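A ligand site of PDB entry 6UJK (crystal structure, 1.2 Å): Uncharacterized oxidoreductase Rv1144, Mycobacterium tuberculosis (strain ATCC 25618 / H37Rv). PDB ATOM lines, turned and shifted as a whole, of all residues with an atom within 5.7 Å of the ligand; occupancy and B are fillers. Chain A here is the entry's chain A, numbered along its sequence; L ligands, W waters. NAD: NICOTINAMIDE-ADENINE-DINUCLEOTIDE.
N of Gly 20 sits at hydrogen-bond distance from O of Val 43. SG of Cys 90 sits at hydrogen-bond distance from OG1 of Thr 149, 3.7 Å away. OG1 of Thr 19 lies within hydrogen-bond range of N of Ala 91 (3.0 Å). NZ of Lys 168 is in hydrogen-bond range of O of Ala 150, at 3.3 Å. The side-chain hydroxyl (OG1) of Thr 199 lies within hydrogen-bond range of the backbone NH (N) of Leu 201, 3.0 Å away. N of Ala 22 is in hydrogen-bond range of OD2 of Asp 44, 3.4 Å away. The backbone NH (N) of Ala 63 lies within hydrogen-bond range of the backbone carbonyl oxygen (O) of Asp 44, at 3.0 Å. The side-chain amino group (NZ) of Lys 168 is in hydrogen-bond range of the backbone carbonyl oxygen (O) of Thr 149 (3.0 Å).
An oxygen (O7N) of the ligand sits at hydrogen-bond distance from the backbone NH of Phe 197, 2.9 Å away. The backbone carbonyl oxygen (O) of Cys 90 sits close to an oxygen (O3D) of the ligand (3.4 Å). OG1 of Thr 199 is in hydrogen-bond range of O1N of the ligand (2.6 Å). O3B of the ligand lies within hydrogen-bond range of OD2 of Asp 44 (2.6 Å). OH of Tyr 164 lies within hydrogen-bond range of O2D of the ligand (2.7 Å). The backbone NH of Val 65 is in hydrogen-bond range of a nitrogen (N1A) of the ligand (3.0 Å). A nitrogen (N6A) of the ligand is in hydrogen-bond range of the side-chain carboxylate of Asp 64 (3.0 Å). The backbone NH of Leu 25 is in hydrogen-bond range of an oxygen (O2N) of the ligand, at 2.8 Å. The side-chain amino group (NZ) of Lys 168 lies within hydrogen-bond range of an oxygen (O3D) of the ligand, 2.9 Å away. N of Gly 24 sits close to O2A of the ligand (3.5 Å). OG of Ser 23 sits at hydrogen-bond distance from O2A of the ligand (2.6 Å).
O7N of the ligand lies close to O of Gly 195, 3.4 Å away. CA of Gly 20 touches O4B of the ligand, at 3.5 Å. Leu 45 touches the ligand. Arg 46 touches the ligand (NH1 to O2B, 3.8 Å). O of Ala 63 touches C2A of the ligand (3.3 Å). Ala 91 touches the ligand (CA to O4B, 3.4 Å). Gly 92 touches the ligand (O to C8A, 3.6 Å). CG2 of Ile 117 touches N7A of the ligand, 3.9 Å away. CG2 of Thr 149 touches O4D of the ligand, at 3.3 Å. Ala 150 touches the ligand (O to C6N, 3.5 Å). Ser 151 touches the ligand (OG to C5N, 3.5 Å). O of Pro 194 touches C5N of the ligand, 3.4 Å away. CA of Leu 196 touches O7N of the ligand (3.8 Å). Pro 200 touches the ligand. Leu 201 touches the ligand. Within 4 Å of the ligand: Gly 20, Ser 23, Gly 24, Leu 25, Asp 44, Leu 45, Arg 46, Ala 63, Asp 64, Val 65, Cys 90, Ala 91, Gly 92, Ile 117, Thr 149, Ala 150, Ser 151, Tyr 164, Lys 168, Pro 194, Gly 195, Leu 196, Phe 197, Thr 199, Pro 200 and Leu 201.
Water W6 bridges O2B of the ligand (2.8 Å) and NH1 of Arg 46 (2.8 Å). Water W9 lies within hydrogen-bond range of an oxygen (O3B) of the ligand (2.8 Å), the backbone carbonyl oxygen (O) of Arg 46 (3.0 Å) and the side-chain carboxylate (OD1) of Asp 44 (3.4 Å). Water W1 lies within hydrogen-bond range of an oxygen (O1A) of the ligand (2.8 Å) and the backbone carbonyl oxygen of Gly 92 (2.9 Å). Water W8 lies within hydrogen-bond range of N of Gly 26 (2.9 Å), O2N of the ligand (2.9 Å), O of Ser 23 (3.0 Å) and O of Gly 20 (3.0 Å).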
ATOM      1  N   THR A  19      20.922  14.603 -27.392  1.00  0.00           N
ATOM      2  CA  THR A  19      21.678  15.284 -26.365  1.00  0.00           C
ATOM      3  C   THR A  19      21.120  14.911 -25.004  1.00  0.00           C
ATOM      4  O   THR A  19      19.918  14.666 -24.856  1.00  0.00           O
ATOM      5  CB  THR A  19      21.692  16.814 -26.520  1.00  0.00           C
ATOM      6  OG1 THR A  19      20.448  17.356 -26.045  1.00  0.00           O
ATOM      7  CG2 THR A  19      21.946  17.243 -27.921  1.00  0.00           C
ATOM      8  N   GLY A  20      21.993  14.864 -24.005  1.00  0.00           N
ATOM      9  CA  GLY A  20      21.561  14.348 -22.718  1.00  0.00           C
ATOM     10  C   GLY A  20      21.192  12.889 -22.754  1.00  0.00           C
ATOM     11  O   GLY A  20      20.514  12.393 -21.858  1.00  0.00           O
ATOM     12  N   GLY A  21      21.671  12.158 -23.776  1.00  0.00           N
ATOM     13  CA  GLY A  21      21.221  10.816 -24.062  1.00  0.00           C
ATOM     14  C   GLY A  21      21.731   9.743 -23.151  1.00  0.00           C
ATOM     15  O   GLY A  21      21.375   8.576 -23.372  1.00  0.00           O
ATOM     16  N   ALA A  22      22.534  10.063 -22.140  1.00  0.00           N
ATOM     17  CA  ALA A  22      23.091   9.069 -21.237  1.00  0.00           C
ATOM     18  C   ALA A  22      22.365   9.006 -19.892  1.00  0.00           C
ATOM     19  O   ALA A  22      22.740   8.197 -19.052  1.00  0.00           O
ATOM     20  CB  ALA A  22      24.578   9.308 -21.002  1.00  0.00           C
ATOM     21  N   SER A  23      21.320   9.809 -19.684  1.00  0.00           N
ATOM     22  CA  SER A  23      20.594   9.791 -18.427  1.00  0.00           C
ATOM     23  C   SER A  23      19.141  10.141 -18.674  1.00  0.00           C
ATOM     24  O   SER A  23      18.815  10.810 -19.664  1.00  0.00           O
ATOM     25  CB  SER A  23      21.197  10.823 -17.460  1.00  0.00           C
ATOM     26  OG  SER A  23      20.594  10.789 -16.181  1.00  0.00           O
ATOM     27  N   GLY A  24      18.255   9.712 -17.766  1.00  0.00           N
ATOM     28  CA  GLY A  24      16.933  10.315 -17.703  1.00  0.00           C
ATOM     29  C   GLY A  24      16.128  10.175 -18.971  1.00  0.00           C
ATOM     30  O   GLY A  24      16.034   9.097 -19.586  1.00  0.00           O
ATOM     31  N   LEU A  25      15.487  11.283 -19.373  1.00  0.00           N
ATOM     32  CA  LEU A  25      14.633  11.258 -20.558  1.00  0.00           C
ATOM     33  C   LEU A  25      15.441  10.942 -21.802  1.00  0.00           C
ATOM     34  O   LEU A  25      14.968  10.214 -22.688  1.00  0.00           O
ATOM     35  CB  LEU A  25      13.944  12.616 -20.706  1.00  0.00           C
ATOM     36  CG  LEU A  25      13.092  13.085 -19.527  1.00  0.00           C
ATOM     37  CD1 LEU A  25      12.392  14.372 -19.878  1.00  0.00           C
ATOM     38  CD2 LEU A  25      12.101  12.011 -19.087  1.00  0.00           C
ATOM     39  N   GLY A  26      16.653  11.501 -21.910  1.00  0.00           N
ATOM     40  CA  GLY A  26      17.466  11.234 -23.074  1.00  0.00           C
ATOM     41  C   GLY A  26      17.868   9.783 -23.192  1.00  0.00           C
ATOM     42  O   GLY A  26      17.903   9.223 -24.291  1.00  0.00           O
ATOM     43  N   VAL A  43      25.092  12.629 -27.212  1.00  0.00           N
ATOM     44  CA  VAL A  43      25.913  13.818 -26.983  1.00  0.00           C
ATOM     45  C   VAL A  43      25.679  14.249 -25.544  1.00  0.00           C
ATOM     46  O   VAL A  43      24.549  14.612 -25.176  1.00  0.00           O
ATOM     47  CB  VAL A  43      25.548  14.918 -27.977  1.00  0.00           C
ATOM     48  CG1 VAL A  43      26.315  16.197 -27.679  1.00  0.00           C
ATOM     49  CG2 VAL A  43      25.803  14.427 -29.416  1.00  0.00           C
ATOM     50  N   ASP A  44      26.713  14.180 -24.716  1.00  0.00           N
ATOM     51  CA  ASP A  44      26.520  14.460 -23.298  1.00  0.00           C
ATOM     52  C   ASP A  44      27.876  14.859 -22.720  1.00  0.00           C
ATOM     53  O   ASP A  44      28.934  14.601 -23.311  1.00  0.00           O
ATOM     54  CB  ASP A  44      25.940  13.203 -22.612  1.00  0.00           C
ATOM     55  CG  ASP A  44      25.162  13.458 -21.344  1.00  0.00           C
ATOM     56  OD1 ASP A  44      25.733  14.063 -20.394  1.00  0.00           O
ATOM     57  OD2 ASP A  44      23.994  12.997 -21.250  1.00  0.00           O
ATOM     58  N   LEU A  45      27.816  15.463 -21.543  1.00  0.00           N
ATOM     59  CA  LEU A  45      29.036  15.744 -20.779  1.00  0.00           C
ATOM     60  C   LEU A  45      29.692  14.465 -20.289  1.00  0.00           C
ATOM     61  O   LEU A  45      30.904  14.437 -20.084  1.00  0.00           O
ATOM     62  CB  LEU A  45      28.692  16.594 -19.562  1.00  0.00           C
ATOM     63  CG  LEU A  45      28.135  17.972 -19.868  1.00  0.00           C
ATOM     64  CD1 LEU A  45      27.652  18.675 -18.614  1.00  0.00           C
ATOM     65  CD2 LEU A  45      29.141  18.836 -20.621  1.00  0.00           C
ATOM     66  N   ARG A  46      28.905  13.422 -20.040  1.00  0.00           N
ATOM     67  CA  ARG A  46      29.391  12.186 -19.441  1.00  0.00           C
ATOM     68  C   ARG A  46      28.386  11.085 -19.735  1.00  0.00           C
ATOM     69  O   ARG A  46      27.275  11.346 -20.211  1.00  0.00           O
ATOM     70  CB  ARG A  46      29.656  12.375 -17.938  1.00  0.00           C
ATOM     71  CG  ARG A  46      28.422  12.705 -17.119  1.00  0.00           C
ATOM     72  CD  ARG A  46      28.788  13.212 -15.702  1.00  0.00           C
ATOM     73  NE  ARG A  46      29.538  14.467 -15.748  1.00  0.00           N
ATOM     74  CZ  ARG A  46      28.985  15.677 -15.735  1.00  0.00           C
ATOM     75  NH1 ARG A  46      27.666  15.811 -15.640  1.00  0.00           N
ATOM     76  NH2 ARG A  46      29.752  16.758 -15.829  1.00  0.00           N
ATOM     77  N   ALA A  63      30.465  16.149 -25.370  1.00  0.00           N
ATOM     78  CA  ALA A  63      30.320  17.520 -25.826  1.00  0.00           C
ATOM     79  C   ALA A  63      29.380  18.252 -24.902  1.00  0.00           C
ATOM     80  O   ALA A  63      28.330  17.739 -24.510  1.00  0.00           O
ATOM     81  CB  ALA A  63      29.763  17.602 -27.245  1.00  0.00           C
ATOM     82  N   ASP A  64      29.770  19.480 -24.610  1.00  0.00           N
ATOM     83  CA  ASP A  64      28.864  20.455 -24.023  1.00  0.00           C
ATOM     84  C   ASP A  64      28.035  21.047 -25.167  1.00  0.00           C
ATOM     85  O   ASP A  64      28.576  21.556 -26.150  1.00  0.00           O
ATOM     86  CB  ASP A  64      29.743  21.522 -23.365  1.00  0.00           C
ATOM     87  CG  ASP A  64      28.973  22.571 -22.623  1.00  0.00           C
ATOM     88  OD1 ASP A  64      27.791  22.862 -22.918  1.00  0.00           O
ATOM     89  OD2 ASP A  64      29.581  23.179 -21.743  1.00  0.00           O
ATOM     90  N   VAL A  65      26.719  20.983 -25.029  1.00  0.00           N
ATOM     91  CA  VAL A  65      25.823  21.453 -26.091  1.00  0.00           C
ATOM     92  C   VAL A  65      25.977  22.944 -26.362  1.00  0.00           C
ATOM     93  O   VAL A  65      25.540  23.416 -27.411  1.00  0.00           O
ATOM     94  CB  VAL A  65      24.334  21.148 -25.797  1.00  0.00           C
ATOM     95  CG1 VAL A  65      24.086  19.658 -25.858  1.00  0.00           C
ATOM     96  CG2 VAL A  65      23.873  21.758 -24.479  1.00  0.00           C
ATOM     97  N   THR A  66      26.597  23.693 -25.450  1.00  0.00           N
ATOM     98  CA  THR A  66      26.813  25.109 -25.688  1.00  0.00           C
ATOM     99  C   THR A  66      28.098  25.407 -26.444  1.00  0.00           C
ATOM    100  O   THR A  66      28.371  26.579 -26.702  1.00  0.00           O
ATOM    101  CB  THR A  66      26.809  25.891 -24.359  1.00  0.00           C
ATOM    102  OG1 THR A  66      27.941  25.528 -23.561  1.00  0.00           O
ATOM    103  CG2 THR A  66      25.532  25.640 -23.563  1.00  0.00           C
ATOM    104  N   ASN A  89      16.780  17.081 -28.394  1.00  0.00           N
ATOM    105  CA  ASN A  89      17.437  17.905 -27.374  1.00  0.00           C
ATOM    106  C   ASN A  89      16.881  17.577 -26.006  1.00  0.00           C
ATOM    107  O   ASN A  89      15.805  18.041 -25.652  1.00  0.00           O
ATOM    108  CB  ASN A  89      17.218  19.388 -27.685  1.00  0.00           C
ATOM    109  CG  ASN A  89      18.083  19.867 -28.813  1.00  0.00           C
ATOM    110  OD1 ASN A  89      19.306  19.882 -28.705  1.00  0.00           O
ATOM    111  ND2 ASN A  89      17.454  20.293 -29.908  1.00  0.00           N
ATOM    112  N   CYS A  90      17.609  16.770 -25.232  1.00  0.00           N
ATOM    113  CA  CYS A  90      17.252  16.460 -23.840  1.00  0.00           C
ATOM    114  C   CYS A  90      18.244  17.024 -22.827  1.00  0.00           C
ATOM    115  O   CYS A  90      17.919  17.083 -21.654  1.00  0.00           O
ATOM    116  CB  CYS A  90      17.084  14.947 -23.597  1.00  0.00           C
ATOM    117  SG  CYS A  90      15.715  14.207 -24.481  1.00  0.00           S
ATOM    118  N   ALA A  91      19.420  17.476 -23.235  1.00  0.00           N
ATOM    119  CA  ALA A  91      20.384  18.003 -22.289  1.00  0.00           C
ATOM    120  C   ALA A  91      19.800  19.228 -21.586  1.00  0.00           C
ATOM    121  O   ALA A  91      19.220  20.115 -22.226  1.00  0.00           O
ATOM    122  CB  ALA A  91      21.642  18.446 -23.042  1.00  0.00           C
ATOM    123  N   GLY A  92      19.988  19.319 -20.274  1.00  0.00           N
ATOM    124  CA  GLY A  92      19.506  20.486 -19.570  1.00  0.00           C
ATOM    125  C   GLY A  92      19.792  20.357 -18.101  1.00  0.00           C
ATOM    126  O   GLY A  92      20.223  19.306 -17.621  1.00  0.00           O
ATOM    127  N   THR A  93      19.512  21.430 -17.391  1.00  0.00           N
ATOM    128  CA  THR A  93      19.694  21.488 -15.953  1.00  0.00           C
ATOM    129  C   THR A  93      18.680  22.452 -15.378  1.00  0.00           C
ATOM    130  O   THR A  93      17.907  23.085 -16.082  1.00  0.00           O
ATOM    131  CB  THR A  93      21.132  21.898 -15.632  1.00  0.00           C
ATOM    132  OG1 THR A  93      21.365  21.759 -14.231  1.00  0.00           O
ATOM    133  CG2 THR A  93      21.383  23.313 -16.044  1.00  0.00           C
ATOM    134  N   ILE A 117      22.496  26.917 -21.039  1.00  0.00           N
ATOM    135  CA  ILE A 117      22.467  25.473 -21.253  1.00  0.00           C
ATOM    136  C   ILE A 117      21.162  25.048 -21.900  1.00  0.00           C
ATOM    137  O   ILE A 117      21.141  24.295 -22.882  1.00  0.00           O
ATOM    138  CB  ILE A 117      22.713  24.748 -19.918  1.00  0.00           C
ATOM    139  CG1 ILE A 117      24.131  25.026 -19.441  1.00  0.00           C
ATOM    140  CG2 ILE A 117      22.440  23.259 -20.057  1.00  0.00           C
ATOM    141  CD1 ILE A 117      24.354  24.699 -17.992  1.00  0.00           C
ATOM    142  N   ASN A 118      20.030  25.499 -21.338  1.00  0.00           N
ATOM    143  CA  ASN A 118      18.747  24.944 -21.718  1.00  0.00           C
ATOM    144  C   ASN A 118      18.219  25.520 -23.014  1.00  0.00           C
ATOM    145  O   ASN A 118      17.550  24.811 -23.786  1.00  0.00           O
ATOM    146  CB  ASN A 118      17.700  25.190 -20.634  1.00  0.00           C
ATOM    147  CG  ASN A 118      17.929  24.371 -19.378  1.00  0.00           C
ATOM    148  OD1 ASN A 118      18.812  23.494 -19.321  1.00  0.00           O
ATOM    149  ND2 ASN A 118      17.118  24.642 -18.363  1.00  0.00           N
ATOM    150  N   THR A 149      13.004  19.540 -25.758  1.00  0.00           N
ATOM    151  CA  THR A 149      12.408  19.340 -24.436  1.00  0.00           C
ATOM    152  C   THR A 149      12.222  20.684 -23.756  1.00  0.00           C
ATOM    153  O   THR A 149      13.200  21.359 -23.416  1.00  0.00           O
ATOM    154  CB  THR A 149      13.238  18.423 -23.560  1.00  0.00           C
ATOM    155  OG1 THR A 149      13.562  17.229 -24.268  1.00  0.00           O
ATOM    156  CG2 THR A 149      12.476  18.053 -22.314  1.00  0.00           C
ATOM    157  N   ALA A 150      10.977  21.087 -23.566  1.00  0.00           N
ATOM    158  CA  ALA A 150      10.658  22.256 -22.743  1.00  0.00           C
ATOM    159  C   ALA A 150      10.352  21.724 -21.338  1.00  0.00           C
ATOM    160  O   ALA A 150      11.170  20.971 -20.790  1.00  0.00           O
ATOM    161  CB  ALA A 150       9.573  23.110 -23.372  1.00  0.00           C
ATOM    162  N   SER A 151       9.204  22.095 -20.784  1.00  0.00           N
ATOM    163  CA  SER A 151       8.770  21.677 -19.455  1.00  0.00           C
ATOM    164  C   SER A 151       7.409  22.319 -19.261  1.00  0.00           C
ATOM    165  O   SER A 151       7.127  23.384 -19.830  1.00  0.00           O
ATOM    166  CB  SER A 151       9.709  22.225 -18.370  1.00  0.00           C
ATOM    167  OG  SER A 151       9.152  22.045 -17.070  1.00  0.00           O
ATOM    168  N   VAL A 152       6.589  21.725 -18.398  1.00  0.00           N
ATOM    169  CA  VAL A 152       5.398  22.435 -17.958  1.00  0.00           C
ATOM    170  C   VAL A 152       5.757  23.758 -17.277  1.00  0.00           C
ATOM    171  O   VAL A 152       4.905  24.636 -17.223  1.00  0.00           O
ATOM    172  CB  VAL A 152       4.525  21.545 -17.029  1.00  0.00           C
ATOM    173  CG1 VAL A 152       3.975  20.344 -17.765  1.00  0.00           C
ATOM    174  CG2 VAL A 152       5.291  21.132 -15.771  1.00  0.00           C
ATOM    175  N   TYR A 164      14.610  28.857 -14.915  1.00  0.00           N
ATOM    176  CA  TYR A 164      14.189  27.631 -15.561  1.00  0.00           C
ATOM    177  C   TYR A 164      13.036  27.903 -16.523  1.00  0.00           C
ATOM    178  O   TYR A 164      13.068  27.500 -17.693  1.00  0.00           O
ATOM    179  CB  TYR A 164      13.830  26.603 -14.493  1.00  0.00           C
ATOM    180  CG  TYR A 164      13.627  25.219 -15.079  1.00  0.00           C
ATOM    181  CD1 TYR A 164      14.717  24.468 -15.562  1.00  0.00           C
ATOM    182  CD2 TYR A 164      12.361  24.646 -15.143  1.00  0.00           C
ATOM    183  CE1 TYR A 164      14.536  23.207 -16.078  1.00  0.00           C
ATOM    184  CE2 TYR A 164      12.186  23.360 -15.672  1.00  0.00           C
ATOM    185  CZ  TYR A 164      13.275  22.654 -16.117  1.00  0.00           C
ATOM    186  OH  TYR A 164      13.094  21.393 -16.633  1.00  0.00           O
ATOM    187  N   LYS A 168      12.814  27.581 -20.636  1.00  0.00           N
ATOM    188  CA  LYS A 168      11.865  26.663 -21.266  1.00  0.00           C
ATOM    189  C   LYS A 168      10.813  27.414 -22.058  1.00  0.00           C
ATOM    190  O   LYS A 168      10.362  26.921 -23.111  1.00  0.00           O
ATOM    191  CB  LYS A 168      11.262  25.744 -20.204  1.00  0.00           C
ATOM    192  CG  LYS A 168      12.314  24.874 -19.511  1.00  0.00           C
ATOM    193  CD  LYS A 168      13.121  24.040 -20.454  1.00  0.00           C
ATOM    194  CE  LYS A 168      13.781  22.865 -19.753  1.00  0.00           C
ATOM    195  NZ  LYS A 168      14.328  21.912 -20.738  1.00  0.00           N
ATOM    196  N   PRO A 194       7.462  18.120 -20.644  1.00  0.00           N
ATOM    197  CA  PRO A 194       7.184  17.113 -19.614  1.00  0.00           C
ATOM    198  C   PRO A 194       6.752  17.735 -18.306  1.00  0.00           C
ATOM    199  O   PRO A 194       7.191  18.834 -17.945  1.00  0.00           O
ATOM    200  CB  PRO A 194       8.520  16.381 -19.432  1.00  0.00           C
ATOM    201  CG  PRO A 194       9.325  16.707 -20.605  1.00  0.00           C
ATOM    202  CD  PRO A 194       8.896  18.103 -21.014  1.00  0.00           C
ATOM    203  N   GLY A 195       5.911  16.992 -17.588  1.00  0.00           N
ATOM    204  CA  GLY A 195       5.623  17.239 -16.194  1.00  0.00           C
ATOM    205  C   GLY A 195       6.654  16.524 -15.352  1.00  0.00           C
ATOM    206  O   GLY A 195       7.840  16.502 -15.682  1.00  0.00           O
ATOM    207  N   LEU A 196       6.210  15.898 -14.286  1.00  0.00           N
ATOM    208  CA  LEU A 196       7.130  15.332 -13.296  1.00  0.00           C
ATOM    209  C   LEU A 196       7.521  13.911 -13.700  1.00  0.00           C
ATOM    210  O   LEU A 196       6.660  13.033 -13.779  1.00  0.00           O
ATOM    211  CB  LEU A 196       6.436  15.310 -11.939  1.00  0.00           C
ATOM    212  CG  LEU A 196       5.974  16.651 -11.361  1.00  0.00           C
ATOM    213  CD1 LEU A 196       5.130  16.495 -10.110  1.00  0.00           C
ATOM    214  CD2 LEU A 196       7.185  17.537 -11.107  1.00  0.00           C
ATOM    215  N   PHE A 197       8.817  13.698 -13.954  1.00  0.00           N
ATOM    216  CA  PHE A 197       9.339  12.394 -14.355  1.00  0.00           C
ATOM    217  C   PHE A 197      10.377  11.902 -13.360  1.00  0.00           C
ATOM    218  O   PHE A 197      11.130  12.694 -12.793  1.00  0.00           O
ATOM    219  CB  PHE A 197       9.941  12.444 -15.776  1.00  0.00           C
ATOM    220  CG  PHE A 197       8.921  12.279 -16.857  1.00  0.00           C
ATOM    221  CD1 PHE A 197       8.041  13.315 -17.174  1.00  0.00           C
ATOM    222  CD2 PHE A 197       8.774  11.057 -17.496  1.00  0.00           C
ATOM    223  CE1 PHE A 197       7.064  13.127 -18.124  1.00  0.00           C
ATOM    224  CE2 PHE A 197       7.801  10.863 -18.465  1.00  0.00           C
ATOM    225  CZ  PHE A 197       6.931  11.894 -18.769  1.00  0.00           C
ATOM    226  N   ASP A 198      10.423  10.596 -13.204  1.00  0.00           N
ATOM    227  CA  ASP A 198      11.390   9.935 -12.326  1.00  0.00           C
ATOM    228  C   ASP A 198      12.725   9.837 -13.045  1.00  0.00           C
ATOM    229  O   ASP A 198      12.997   8.875 -13.770  1.00  0.00           O
ATOM    230  CB  ASP A 198      10.868   8.563 -11.945  1.00  0.00           C
ATOM    231  CG  ASP A 198      11.705   7.905 -10.875  1.00  0.00           C
ATOM    232  OD1 ASP A 198      12.753   8.458 -10.486  1.00  0.00           O
ATOM    233  OD2 ASP A 198      11.285   6.828 -10.424  1.00  0.00           O
ATOM    234  N   THR A 199      13.553  10.847 -12.875  1.00  0.00           N
ATOM    235  CA  THR A 199      14.898  10.858 -13.467  1.00  0.00           C
ATOM    236  C   THR A 199      15.872  11.338 -12.409  1.00  0.00           C
ATOM    237  O   THR A 199      15.460  11.863 -11.364  1.00  0.00           O
ATOM    238  CB  THR A 199      15.012  11.830 -14.649  1.00  0.00           C
ATOM    239  OG1 THR A 199      14.988  13.159 -14.152  1.00  0.00           O
ATOM    240  CG2 THR A 199      13.940  11.596 -15.693  1.00  0.00           C
ATOM    241  N   PRO A 200      17.168  11.240 -12.668  1.00  0.00           N
ATOM    242  CA  PRO A 200      18.167  11.822 -11.765  1.00  0.00           C
ATOM    243  C   PRO A 200      18.012  13.321 -11.553  1.00  0.00           C
ATOM    244  O   PRO A 200      18.630  13.851 -10.626  1.00  0.00           O
ATOM    245  CB  PRO A 200      19.495  11.468 -12.446  1.00  0.00           C
ATOM    246  CG  PRO A 200      19.174  10.181 -13.165  1.00  0.00           C
ATOM    247  CD  PRO A 200      17.793  10.388 -13.705  1.00  0.00           C
ATOM    248  N   LEU A 201      17.247  14.029 -12.386  1.00  0.00           N
ATOM    249  CA  LEU A 201      17.012  15.453 -12.140  1.00  0.00           C
ATOM    250  C   LEU A 201      16.393  15.683 -10.767  1.00  0.00           C
ATOM    251  O   LEU A 201      16.627  16.719 -10.151  1.00  0.00           O
ATOM    252  CB  LEU A 201      16.098  16.032 -13.218  1.00  0.00           C
ATOM    253  CG  LEU A 201      15.782  17.527 -13.134  1.00  0.00           C
ATOM    254  CD1 LEU A 201      17.022  18.384 -13.386  1.00  0.00           C
ATOM    255  CD2 LEU A 201      14.700  17.879 -14.143  1.00  0.00           C
ATOM    256  N   LEU A 202      15.622  14.714 -10.275  1.00  0.00           N
ATOM    257  CA  LEU A 202      15.005  14.797  -8.961  1.00  0.00           C
ATOM    258  C   LEU A 202      15.848  14.156  -7.874  1.00  0.00           C
ATOM    259  O   LEU A 202      15.309  13.776  -6.825  1.00  0.00           O
ATOM    260  CB  LEU A 202      13.617  14.146  -8.976  1.00  0.00           C
ATOM    261  CG  LEU A 202      12.618  14.713  -9.989  1.00  0.00           C
ATOM    262  CD1 LEU A 202      11.270  14.035  -9.820  1.00  0.00           C
ATOM    263  CD2 LEU A 202      12.498  16.213  -9.825  1.00  0.00           C
HETATM  264  PA  NAD L   1      19.010  14.129 -16.272  1.00  0.00           P
HETATM  265  O1A NAD L   1      19.831  14.950 -15.365  1.00  0.00           O
HETATM  266  O2A NAD L   1      18.755  12.673 -15.974  1.00  0.00           O
HETATM  267  O5B NAD L   1      19.574  14.187 -17.744  1.00  0.00           O
HETATM  268  C5B NAD L   1      20.121  15.397 -18.303  1.00  0.00           C
HETATM  269  C4B NAD L   1      21.334  15.005 -19.105  1.00  0.00           C
HETATM  270  O4B NAD L   1      21.821  16.197 -19.751  1.00  0.00           O
HETATM  271  C3B NAD L   1      22.493  14.426 -18.266  1.00  0.00           C
HETATM  272  O3B NAD L   1      23.011  13.211 -18.813  1.00  0.00           O
HETATM  273  C2B NAD L   1      23.514  15.577 -18.272  1.00  0.00           C
HETATM  274  O2B NAD L   1      24.859  15.156 -18.156  1.00  0.00           O
HETATM  275  C1B NAD L   1      23.224  16.224 -19.631  1.00  0.00           C
HETATM  276  N9A NAD L   1      23.683  17.598 -19.757  1.00  0.00           N
HETATM  277  C8A NAD L   1      23.488  18.633 -18.884  1.00  0.00           C
HETATM  278  N7A NAD L   1      24.045  19.764 -19.269  1.00  0.00           N
HETATM  279  C5A NAD L   1      24.659  19.431 -20.472  1.00  0.00           C
HETATM  280  C6A NAD L   1      25.443  20.178 -21.369  1.00  0.00           C
HETATM  281  N6A NAD L   1      25.780  21.461 -21.176  1.00  0.00           N
HETATM  282  N1A NAD L   1      25.882  19.545 -22.492  1.00  0.00           N
HETATM  283  C2A NAD L   1      25.615  18.254 -22.650  1.00  0.00           C
HETATM  284  N3A NAD L   1      24.912  17.444 -21.849  1.00  0.00           N
HETATM  285  C4A NAD L   1      24.453  18.098 -20.778  1.00  0.00           C
HETATM  286  O3  NAD L   1      17.623  14.861 -16.333  1.00  0.00           O
HETATM  287  PN  NAD L   1      16.298  14.705 -17.217  1.00  0.00           P
HETATM  288  O1N NAD L   1      15.167  14.707 -16.279  1.00  0.00           O
HETATM  289  O2N NAD L   1      16.446  13.588 -18.186  1.00  0.00           O
HETATM  290  O5D NAD L   1      16.334  16.038 -18.026  1.00  0.00           O
HETATM  291  C5D NAD L   1      16.070  15.910 -19.442  1.00  0.00           C
HETATM  292  C4D NAD L   1      15.380  17.154 -19.925  1.00  0.00           C
HETATM  293  O4D NAD L   1      13.997  17.139 -19.485  1.00  0.00           O
HETATM  294  C3D NAD L   1      15.980  18.448 -19.380  1.00  0.00           C
HETATM  295  O3D NAD L   1      15.872  19.441 -20.399  1.00  0.00           O
HETATM  296  C2D NAD L   1      15.041  18.798 -18.229  1.00  0.00           C
HETATM  297  O2D NAD L   1      15.073  20.210 -17.984  1.00  0.00           O
HETATM  298  C1D NAD L   1      13.718  18.341 -18.837  1.00  0.00           C
HETATM  299  N1N NAD L   1      12.585  18.111 -17.858  1.00  0.00           N
HETATM  300  C2N NAD L   1      12.679  17.134 -16.942  1.00  0.00           C
HETATM  301  C3N NAD L   1      11.663  16.957 -16.016  1.00  0.00           C
HETATM  302  C7N NAD L   1      11.665  15.832 -15.024  1.00  0.00           C
HETATM  303  O7N NAD L   1      10.784  15.777 -14.149  1.00  0.00           O
HETATM  304  N7N NAD L   1      12.646  14.933 -15.105  1.00  0.00           N
HETATM  305  C4N NAD L   1      10.557  17.823 -16.069  1.00  0.00           C
HETATM  306  C5N NAD L   1      10.497  18.809 -17.036  1.00  0.00           C
HETATM  307  C6N NAD L   1      11.530  18.934 -17.932  1.00  0.00           C
HETATM  308  O   HOH W   1      20.289  17.699 -15.249  1.00  0.00           O
HETATM  309  O   HOH W   2      25.040  21.362 -17.196  1.00  0.00           O
HETATM  310  O   HOH W   3      23.020  17.768 -15.586  1.00  0.00           O
HETATM  311  O   HOH W   4      10.768  18.150 -12.563  1.00  0.00           O
HETATM  312  O   HOH W   5      27.268  22.695 -18.578  1.00  0.00           O
HETATM  313  O   HOH W   6      25.474  14.117 -15.684  1.00  0.00           O
HETATM  314  O   HOH W   7      16.653  19.969 -23.165  1.00  0.00           O
HETATM  315  O   HOH W   8      18.094  13.543 -20.528  1.00  0.00           O
HETATM  316  O   HOH W   9      25.140  11.554 -18.139  1.00  0.00           O
HETATM  317  O   HOH W  10      21.731  14.196 -13.623  1.00  0.00           O
